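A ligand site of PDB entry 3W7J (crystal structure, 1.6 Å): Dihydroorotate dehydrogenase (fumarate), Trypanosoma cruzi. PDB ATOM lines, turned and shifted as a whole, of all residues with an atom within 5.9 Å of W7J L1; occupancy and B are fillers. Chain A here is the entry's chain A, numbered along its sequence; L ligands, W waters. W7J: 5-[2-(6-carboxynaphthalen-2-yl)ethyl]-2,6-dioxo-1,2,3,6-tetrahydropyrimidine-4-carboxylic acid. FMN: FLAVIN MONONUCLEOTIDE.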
ATOM      1  N   LYS A  44      -1.051   0.337 -26.691  1.00  0.00           N
ATOM      2  CA  LYS A  44      -0.361   1.071 -25.698  1.00  0.00           C
ATOM      3  C   LYS A  44      -1.325   1.818 -24.772  1.00  0.00           C
ATOM      4  O   LYS A  44      -2.259   2.461 -25.254  1.00  0.00           O
ATOM      5  CB  LYS A  44       0.538   2.085 -26.387  1.00  0.00           C
ATOM      6  CG  LYS A  44       1.129   3.100 -25.422  1.00  0.00           C
ATOM      7  CD  LYS A  44       2.241   2.638 -24.455  1.00  0.00           C
ATOM      8  CE  LYS A  44       2.515   3.600 -23.244  1.00  0.00           C
ATOM      9  NZ  LYS A  44       3.671   3.240 -22.228  1.00  0.00           N
ATOM     10  N   SER A  45      -1.023   1.770 -23.482  1.00  0.00           N
ATOM     11  CA  SER A  45      -1.867   2.493 -22.484  1.00  0.00           C
ATOM     12  C   SER A  45      -2.009   3.914 -22.986  1.00  0.00           C
ATOM     13  O   SER A  45      -1.029   4.548 -23.264  1.00  0.00           O
ATOM     14  CB  SER A  45      -1.355   2.471 -21.116  1.00  0.00           C
ATOM     15  OG  SER A  45      -1.395   1.101 -20.675  1.00  0.00           O
ATOM     16  N   ARG A  51       0.746  12.186 -25.535  1.00  0.00           N
ATOM     17  CA  ARG A  51       1.869  12.532 -24.670  1.00  0.00           C
ATOM     18  C   ARG A  51       3.170  12.163 -25.331  1.00  0.00           C
ATOM     19  O   ARG A  51       3.310  11.108 -25.930  1.00  0.00           O
ATOM     20  CB  ARG A  51       1.842  11.723 -23.352  1.00  0.00           C
ATOM     21  CG  ARG A  51       0.683  12.087 -22.435  1.00  0.00           C
ATOM     22  CD  ARG A  51       0.568  11.127 -21.278  1.00  0.00           C
ATOM     23  NE  ARG A  51       1.785  11.075 -20.481  1.00  0.00           N
ATOM     24  CZ  ARG A  51       2.043  11.902 -19.469  1.00  0.00           C
ATOM     25  NH1 ARG A  51       1.218  12.927 -19.174  1.00  0.00           N
ATOM     26  NH2 ARG A  51       3.158  11.749 -18.772  1.00  0.00           N
ATOM     27  N   ASN A  54       8.578  10.804 -21.177  1.00  0.00           N
ATOM     28  CA  ASN A  54       9.733  11.338 -20.475  1.00  0.00           C
ATOM     29  C   ASN A  54      10.962  11.480 -21.354  1.00  0.00           C
ATOM     30  O   ASN A  54      11.021  10.919 -22.447  1.00  0.00           O
ATOM     31  CB  ASN A  54      10.052  10.395 -19.346  1.00  0.00           C
ATOM     32  CG  ASN A  54       9.167  10.550 -18.174  1.00  0.00           C
ATOM     33  OD1 ASN A  54       8.458  11.562 -17.999  1.00  0.00           O
ATOM     34  ND2 ASN A  54       9.147   9.550 -17.296  1.00  0.00           N
ATOM     35  N   ASN A  68      12.460   0.838 -17.028  1.00  0.00           N
ATOM     36  CA  ASN A  68      11.868   1.885 -17.860  1.00  0.00           C
ATOM     37  C   ASN A  68      11.233   2.945 -16.972  1.00  0.00           C
ATOM     38  O   ASN A  68      10.600   2.671 -15.960  1.00  0.00           O
ATOM     39  CB  ASN A  68      10.894   1.343 -18.891  1.00  0.00           C
ATOM     40  CG  ASN A  68       9.512   1.172 -18.358  1.00  0.00           C
ATOM     41  OD1 ASN A  68       8.748   2.159 -18.295  1.00  0.00           O
ATOM     42  ND2 ASN A  68       9.172  -0.028 -17.936  1.00  0.00           N
ATOM     43  N   SER A  69      11.274   4.164 -17.455  1.00  0.00           N
ATOM     44  CA  SER A  69      10.408   5.233 -16.983  1.00  0.00           C
ATOM     45  C   SER A  69       9.946   5.936 -18.242  1.00  0.00           C
ATOM     46  O   SER A  69      10.321   7.075 -18.500  1.00  0.00           O
ATOM     47  CB  SER A  69      11.112   6.153 -16.015  1.00  0.00           C
ATOM     48  OG  SER A  69      10.265   7.209 -15.542  1.00  0.00           O
ATOM     49  N   MET A  70       9.131   5.254 -19.038  1.00  0.00           N
ATOM     50  CA  MET A  70       8.640   5.843 -20.265  1.00  0.00           C
ATOM     51  C   MET A  70       7.854   7.132 -20.088  1.00  0.00           C
ATOM     52  O   MET A  70       7.979   8.092 -20.898  1.00  0.00           O
ATOM     53  CB  MET A  70       7.838   4.878 -21.042  1.00  0.00           C
ATOM     54  CG  MET A  70       8.425   3.562 -21.424  1.00  0.00           C
ATOM     55  SD  MET A  70       9.982   3.642 -22.292  1.00  0.00           S
ATOM     56  CE  MET A  70       9.432   4.146 -23.865  1.00  0.00           C
ATOM     57  N   GLY A  71       7.020   7.178 -19.062  1.00  0.00           N
ATOM     58  CA  GLY A  71       6.199   8.345 -18.800  1.00  0.00           C
ATOM     59  C   GLY A  71       4.942   8.367 -19.651  1.00  0.00           C
ATOM     60  O   GLY A  71       4.471   9.448 -20.039  1.00  0.00           O
ATOM     61  N   LEU A  72       4.449   7.223 -20.056  1.00  0.00           N
ATOM     62  CA  LEU A  72       3.241   7.118 -20.790  1.00  0.00           C
ATOM     63  C   LEU A  72       3.223   7.882 -22.103  1.00  0.00           C
ATOM     64  O   LEU A  72       2.186   8.521 -22.453  1.00  0.00           O
ATOM     65  CB  LEU A  72       2.046   7.472 -19.888  1.00  0.00           C
ATOM     66  CG  LEU A  72       0.644   6.904 -20.173  1.00  0.00           C
ATOM     67  CD1 LEU A  72       0.610   5.435 -20.501  1.00  0.00           C
ATOM     68  CD2 LEU A  72      -0.164   7.172 -18.890  1.00  0.00           C
ATOM     69  N   PRO A  73       4.225   7.746 -22.926  1.00  0.00           N
ATOM     70  CA  PRO A  73       4.140   8.310 -24.282  1.00  0.00           C
ATOM     71  C   PRO A  73       3.072   7.564 -25.047  1.00  0.00           C
ATOM     72  O   PRO A  73       3.019   6.334 -24.973  1.00  0.00           O
ATOM     73  CB  PRO A  73       5.487   8.053 -24.865  1.00  0.00           C
ATOM     74  CG  PRO A  73       6.014   6.865 -24.195  1.00  0.00           C
ATOM     75  CD  PRO A  73       5.399   6.853 -22.813  1.00  0.00           C
ATOM     76  N   SER A 100      -4.973   4.294 -19.456  1.00  0.00           N
ATOM     77  CA  SER A 100      -4.275   4.610 -18.262  1.00  0.00           C
ATOM     78  C   SER A 100      -4.385   6.079 -17.992  1.00  0.00           C
ATOM     79  O   SER A 100      -3.376   6.857 -17.887  1.00  0.00           O
ATOM     80  CB  SER A 100      -2.872   4.112 -18.425  1.00  0.00           C
ATOM     81  OG  SER A 100      -2.110   4.364 -17.258  1.00  0.00           O
ATOM     82  N   LEU A 102      -4.810   9.569 -16.048  1.00  0.00           N
ATOM     83  CA  LEU A 102      -4.028  10.072 -14.904  1.00  0.00           C
ATOM     84  C   LEU A 102      -4.908  10.544 -13.725  1.00  0.00           C
ATOM     85  O   LEU A 102      -4.391  11.063 -12.706  1.00  0.00           O
ATOM     86  CB  LEU A 102      -2.908  11.096 -15.329  1.00  0.00           C
ATOM     87  CG  LEU A 102      -1.909  10.348 -16.284  1.00  0.00           C
ATOM     88  CD1 LEU A 102      -0.980  11.277 -16.934  1.00  0.00           C
ATOM     89  CD2 LEU A 102      -1.028   9.388 -15.531  1.00  0.00           C
ATOM     90  N   ASN A 128      -5.457   0.136 -16.762  1.00  0.00           N
ATOM     91  CA  ASN A 128      -4.205   0.076 -15.990  1.00  0.00           C
ATOM     92  C   ASN A 128      -4.319   0.771 -14.689  1.00  0.00           C
ATOM     93  O   ASN A 128      -4.506   1.956 -14.630  1.00  0.00           O
ATOM     94  CB  ASN A 128      -3.054   0.728 -16.773  1.00  0.00           C
ATOM     95  CG  ASN A 128      -1.718   0.588 -16.044  1.00  0.00           C
ATOM     96  OD1 ASN A 128      -1.471  -0.255 -15.208  1.00  0.00           O
ATOM     97  ND2 ASN A 128      -0.853   1.495 -16.377  1.00  0.00           N
ATOM     98  N   SER A 130      -1.766   0.364 -12.322  1.00  0.00           N
ATOM     99  CA  SER A 130      -0.421   0.600 -11.861  1.00  0.00           C
ATOM    100  C   SER A 130      -0.028   1.830 -12.496  1.00  0.00           C
ATOM    101  O   SER A 130       0.772   1.795 -13.447  1.00  0.00           O
ATOM    102  CB  SER A 130       0.522  -0.501 -12.288  1.00  0.00           C
ATOM    103  OG  SER A 130       1.843  -0.314 -11.777  1.00  0.00           O
ATOM    104  N   CYS A 131      -0.529   2.949 -12.016  1.00  0.00           N
ATOM    105  CA  CYS A 131      -0.505   4.189 -12.697  1.00  0.00           C
ATOM    106  C   CYS A 131      -0.436   5.284 -11.575  1.00  0.00           C
ATOM    107  O   CYS A 131      -1.143   5.219 -10.533  1.00  0.00           O
ATOM    108  CB  CYS A 131      -1.897   4.327 -13.383  1.00  0.00           C
ATOM    109  SG  CYS A 131      -1.984   5.759 -14.484  1.00  0.00           S
ATOM    110  N   PRO A 132       0.243   6.397 -11.811  1.00  0.00           N
ATOM    111  CA  PRO A 132       0.117   7.549 -10.964  1.00  0.00           C
ATOM    112  C   PRO A 132      -1.275   8.107 -10.822  1.00  0.00           C
ATOM    113  O   PRO A 132      -2.039   8.102 -11.751  1.00  0.00           O
ATOM    114  CB  PRO A 132       1.056   8.600 -11.622  1.00  0.00           C
ATOM    115  CG  PRO A 132       1.900   7.843 -12.520  1.00  0.00           C
ATOM    116  CD  PRO A 132       1.172   6.604 -12.916  1.00  0.00           C
ATOM    117  N   LYS A 165      -5.113  -4.198 -15.144  1.00  0.00           N
ATOM    118  CA  LYS A 165      -3.672  -4.493 -15.057  1.00  0.00           C
ATOM    119  C   LYS A 165      -3.152  -4.072 -13.684  1.00  0.00           C
ATOM    120  O   LYS A 165      -3.302  -2.898 -13.254  1.00  0.00           O
ATOM    121  CB  LYS A 165      -2.948  -3.669 -16.132  1.00  0.00           C
ATOM    122  CG  LYS A 165      -1.417  -3.865 -16.170  1.00  0.00           C
ATOM    123  CD  LYS A 165      -0.965  -5.185 -16.757  1.00  0.00           C
ATOM    124  CE  LYS A 165       0.493  -5.284 -17.140  1.00  0.00           C
ATOM    125  NZ  LYS A 165       0.868  -4.456 -18.251  1.00  0.00           N
ATOM    126  N   ASN A 195       2.127  -5.799 -13.814  1.00  0.00           N
ATOM    127  CA  ASN A 195       2.936  -4.646 -14.324  1.00  0.00           C
ATOM    128  C   ASN A 195       4.427  -4.723 -13.824  1.00  0.00           C
ATOM    129  O   ASN A 195       4.770  -5.615 -12.994  1.00  0.00           O
ATOM    130  CB  ASN A 195       2.265  -3.323 -13.939  1.00  0.00           C
ATOM    131  CG  ASN A 195       2.448  -2.254 -15.007  1.00  0.00           C
ATOM    132  OD1 ASN A 195       3.604  -1.956 -15.385  1.00  0.00           O
ATOM    133  ND2 ASN A 195       1.358  -1.621 -15.448  1.00  0.00           N
ATOM    134  N   SER A 196       5.238  -3.774 -14.205  1.00  0.00           N
ATOM    135  CA  SER A 196       6.617  -3.798 -13.775  1.00  0.00           C
ATOM    136  C   SER A 196       6.803  -3.702 -12.253  1.00  0.00           C
ATOM    137  O   SER A 196       6.031  -3.198 -11.596  1.00  0.00           O
ATOM    138  CB  SER A 196       7.414  -2.704 -14.547  1.00  0.00           C
ATOM    139  OG  SER A 196       6.788  -1.523 -14.443  1.00  0.00           O
ATOM    140  N   PRO A 214      15.071   9.793 -16.538  1.00  0.00           N
ATOM    141  CA  PRO A 214      14.036  10.287 -15.627  1.00  0.00           C
ATOM    142  C   PRO A 214      14.205   9.765 -14.214  1.00  0.00           C
ATOM    143  O   PRO A 214      14.838   8.744 -14.027  1.00  0.00           O
ATOM    144  CB  PRO A 214      12.743   9.770 -16.238  1.00  0.00           C
ATOM    145  CG  PRO A 214      13.076   9.378 -17.659  1.00  0.00           C
ATOM    146  CD  PRO A 214      14.499   8.963 -17.609  1.00  0.00           C
ATOM    147  N   LYS A 215      13.549  10.493 -13.338  1.00  0.00           N
ATOM    148  CA  LYS A 215      13.486  10.030 -11.996  1.00  0.00           C
ATOM    149  C   LYS A 215      14.834   9.475 -11.205  1.00  0.00           C
ATOM    150  O   LYS A 215      14.958   8.597 -10.357  1.00  0.00           O
ATOM    151  CB  LYS A 215      12.494   8.856 -11.872  1.00  0.00           C
ATOM    152  CG  LYS A 215      11.042   9.231 -12.115  1.00  0.00           C
ATOM    153  CD  LYS A 215      10.200   7.928 -12.092  1.00  0.00           C
ATOM    154  CE  LYS A 215       9.715   7.181 -10.809  1.00  0.00           C
ATOM    155  NZ  LYS A 215      10.368   6.974  -9.468  1.00  0.00           N
ATOM    156  N   GLY A 220      10.609   1.134 -13.569  1.00  0.00           N
ATOM    157  CA  GLY A 220      10.007  -0.149 -13.393  1.00  0.00           C
ATOM    158  C   GLY A 220      10.801  -1.263 -14.051  1.00  0.00           C
ATOM    159  O   GLY A 220      11.330  -1.183 -15.134  1.00  0.00           O
HETATM  160  OAJ W7J L   1       6.337   4.532 -17.934  1.00  0.00           O
HETATM  161  CAI W7J L   1       5.352   4.041 -18.476  1.00  0.00           C
HETATM  162  OAK W7J L   1       4.742   4.555 -19.440  1.00  0.00           O
HETATM  163  C4  W7J L   1       4.863   2.770 -17.882  1.00  0.00           C
HETATM  164  N3  W7J L   1       5.863   1.807 -17.694  1.00  0.00           N
HETATM  165  C2  W7J L   1       5.568   0.580 -17.127  1.00  0.00           C
HETATM  166  O2  W7J L   1       6.461  -0.242 -16.852  1.00  0.00           O
HETATM  167  N1  W7J L   1       4.304   0.362 -16.786  1.00  0.00           N
HETATM  168  C6  W7J L   1       3.220   1.260 -17.013  1.00  0.00           C
HETATM  169  O6  W7J L   1       2.092   0.960 -16.636  1.00  0.00           O
HETATM  170  C5  W7J L   1       3.550   2.487 -17.593  1.00  0.00           C
HETATM  171  CAL W7J L   1       2.480   3.443 -17.732  1.00  0.00           C
HETATM  172  CAM W7J L   1       1.990   4.205 -16.360  1.00  0.00           C
HETATM  173  CAN W7J L   1       2.816   5.370 -16.049  1.00  0.00           C
HETATM  174  CAO W7J L   1       2.400   6.707 -16.229  1.00  0.00           C
HETATM  175  CAP W7J L   1       3.377   7.718 -15.890  1.00  0.00           C
HETATM  176  CAT W7J L   1       3.156   9.034 -16.163  1.00  0.00           C
HETATM  177  CAU W7J L   1       4.135   9.975 -15.813  1.00  0.00           C
HETATM  178  CAV W7J L   1       5.393   9.639 -15.283  1.00  0.00           C
HETATM  179  CAX W7J L   1       6.384  10.634 -14.914  1.00  0.00           C
HETATM  180  OAZ W7J L   1       5.934  11.817 -14.874  1.00  0.00           O
HETATM  181  OAY W7J L   1       7.639  10.379 -14.759  1.00  0.00           O
HETATM  182  CAW W7J L   1       5.652   8.369 -15.078  1.00  0.00           C
HETATM  183  CAQ W7J L   1       4.664   7.415 -15.444  1.00  0.00           C
HETATM  184  CAR W7J L   1       4.999   6.177 -15.163  1.00  0.00           C
HETATM  185  CAS W7J L   1       4.085   5.172 -15.522  1.00  0.00           C
HETATM  186  N1  FMN L   2       2.288  -1.628 -18.727  1.00  0.00           N
HETATM  187  C2  FMN L   2       1.097  -1.086 -18.937  1.00  0.00           C
HETATM  188  O2  FMN L   2       0.082  -1.611 -18.480  1.00  0.00           O
HETATM  189  N3  FMN L   2       0.931  -0.038 -19.755  1.00  0.00           N
HETATM  190  C4  FMN L   2       1.972   0.519 -20.424  1.00  0.00           C
HETATM  191  O4  FMN L   2       1.817   1.527 -21.210  1.00  0.00           O
HETATM  192  C4A FMN L   2       3.255  -0.009 -20.206  1.00  0.00           C
HETATM  193  N5  FMN L   2       4.318   0.472 -20.887  1.00  0.00           N
HETATM  194  C5A FMN L   2       5.505  -0.237 -20.833  1.00  0.00           C
HETATM  195  C6  FMN L   2       6.581   0.183 -21.621  1.00  0.00           C
HETATM  196  C7  FMN L   2       7.769  -0.468 -21.669  1.00  0.00           C
HETATM  197  C7M FMN L   2       8.946  -0.017 -22.474  1.00  0.00           C
HETATM  198  C8  FMN L   2       7.929  -1.625 -20.780  1.00  0.00           C
HETATM  199  C8M FMN L   2       9.174  -2.393 -20.747  1.00  0.00           C
HETATM  200  C9  FMN L   2       6.898  -2.014 -19.984  1.00  0.00           C
HETATM  201  C9A FMN L   2       5.657  -1.391 -19.973  1.00  0.00           C
HETATM  202  N10 FMN L   2       4.544  -1.813 -19.206  1.00  0.00           N
HETATM  203  C10 FMN L   2       3.355  -1.189 -19.365  1.00  0.00           C
HETATM  204  C1' FMN L   2       4.650  -2.992 -18.395  1.00  0.00           C
HETATM  205  C2' FMN L   2       4.560  -4.278 -19.215  1.00  0.00           C
HETATM  206  O2' FMN L   2       3.270  -4.319 -19.782  1.00  0.00           O
HETATM  207  C3' FMN L   2       4.816  -5.468 -18.344  1.00  0.00           C
HETATM  208  O3' FMN L   2       3.751  -5.462 -17.336  1.00  0.00           O
HETATM  209  C4' FMN L   2       6.176  -5.471 -17.636  1.00  0.00           C
HETATM  210  O4' FMN L   2       7.170  -5.060 -18.566  1.00  0.00           O
HETATM  211  C5' FMN L   2       6.527  -6.934 -17.156  1.00  0.00           C
HETATM  212  O5' FMN L   2       6.492  -7.899 -18.195  1.00  0.00           O
HETATM  213  P   FMN L   2       7.939  -8.413 -18.754  1.00  0.00           P
HETATM  214  O1P FMN L   2       7.540  -9.375 -19.862  1.00  0.00           O
HETATM  215  O2P FMN L   2       8.714  -8.980 -17.606  1.00  0.00           O
HETATM  216  O3P FMN L   2       8.687  -7.139 -19.247  1.00  0.00           O
HETATM  217  O   HOH W   1       4.594  13.328 -16.836  1.00  0.00           O
HETATM  218  O   HOH W   2       7.717   3.512 -15.654  1.00  0.00           O
HETATM  219  O   HOH W   3       3.501   1.566 -13.679  1.00  0.00           O
HETATM  220  O   HOH W   4       9.461  12.410 -14.789  1.00  0.00           O
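OG of Ser 196 is in hydrogen-bond range of O2 of W7J L1, at 2.7 Å.
OAK of W7J L1 is in hydrogen-bond range of N of Leu 72, 2.8 Å away.
A nitrogen (N1) of W7J L1 lies within hydrogen-bond range of the side-chain amide oxygen (OD1) of Asn 195 (2.8 Å).
ND2 of Asn 68 is in hydrogen-bond range of O2 of W7J L1, at 2.9 Å.
OAJ of W7J L1 is in hydrogen-bond range of N of Gly 71 (3.0 Å).
O6 of W7J L1 sits at hydrogen-bond distance from ND2 of Asn 128 (3.0 Å).
An oxygen (OAY) of W7J L1 lies within hydrogen-bond range of the side-chain amide nitrogen (ND2) of Asn 54 (3.1 Å).
N of Met 70 is in hydrogen-bond range of OAJ of W7J L1, at 3.1 Å.
An oxygen (OAK) of W7J L1 lies within salt-bridge range of the side-chain amino group (NZ) of Lys 44 (3.3 Å).
An oxygen (O2) of FMN L2 sits at hydrogen-bond distance from the side-chain amide nitrogen (ND2) of Asn 195 (3.3 Å).
NZ of Lys 44 sits at hydrogen-bond distance from O4 of FMN L2, 2.7 Å away.
OG of Ser 45 lies within hydrogen-bond range of N3 of FMN L2 (2.7 Å).
The side-chain amino group of Lys 165 is in hydrogen-bond range of an oxygen (O2') of FMN L2 (2.9 Å).
A nitrogen (N1) of FMN L2 sits close to a nitrogen (N1) of W7J L1 (3.4 Å).
OD1 of Asn 195 lies within hydrogen-bond range of OG of Ser 196 (3.3 Å).
The guanidinium group (NE) of Arg 51 is in hydrogen-bond range of the backbone carbonyl oxygen (O) of Leu 72, 3.3 Å away.
The side-chain amide nitrogen (ND2) of Asn 195 sits at hydrogen-bond distance from the side-chain amide oxygen (OD1) of Asn 128 (3.2 Å).
The side-chain amide oxygen of Asn 68 is in hydrogen-bond range of the backbone NH of Met 70 (3.2 Å).
The guanidinium group (NH2) of Arg 51 is in hydrogen-bond range of the backbone carbonyl oxygen (O) of Gly 71 (2.9 Å).
The side-chain amide nitrogen of Asn 128 lies within hydrogen-bond range of the side-chain hydroxyl of Ser 100, at 3.3 Å.
O of Met 70 lies within hydrogen-bond range of N of Asn 54.
The side-chain amide nitrogen (ND2) of Asn 54 is in hydrogen-bond range of the backbone carbonyl oxygen (O) of Ser 69, 3.0 Å away.
Merely in contact with W7J L1: Pro 132, Ser 130, Arg 51 and Ser 69.
Hydrophobic or aromatic side chains within 4 Å of W7J L1: Met 70, Leu 72 and Pro 132.
Water W4 lies within hydrogen-bond range of OAY of W7J L1 and OD1 of Asn 54.
Water W1 bridges OAZ of W7J L1 (2.8 Å) and NH2 of Arg 51 (2.9 Å).
Water W2 lies within hydrogen-bond range of an oxygen (OAJ) of W7J L1 (2.9 Å) and the backbone carbonyl oxygen of Asn 68 (3.0 Å).
Water W3 lies within hydrogen-bond range of the backbone carbonyl oxygen (O) of Ser 130 (2.7 Å) and an oxygen (O6) of W7J L1 (3.3 Å).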
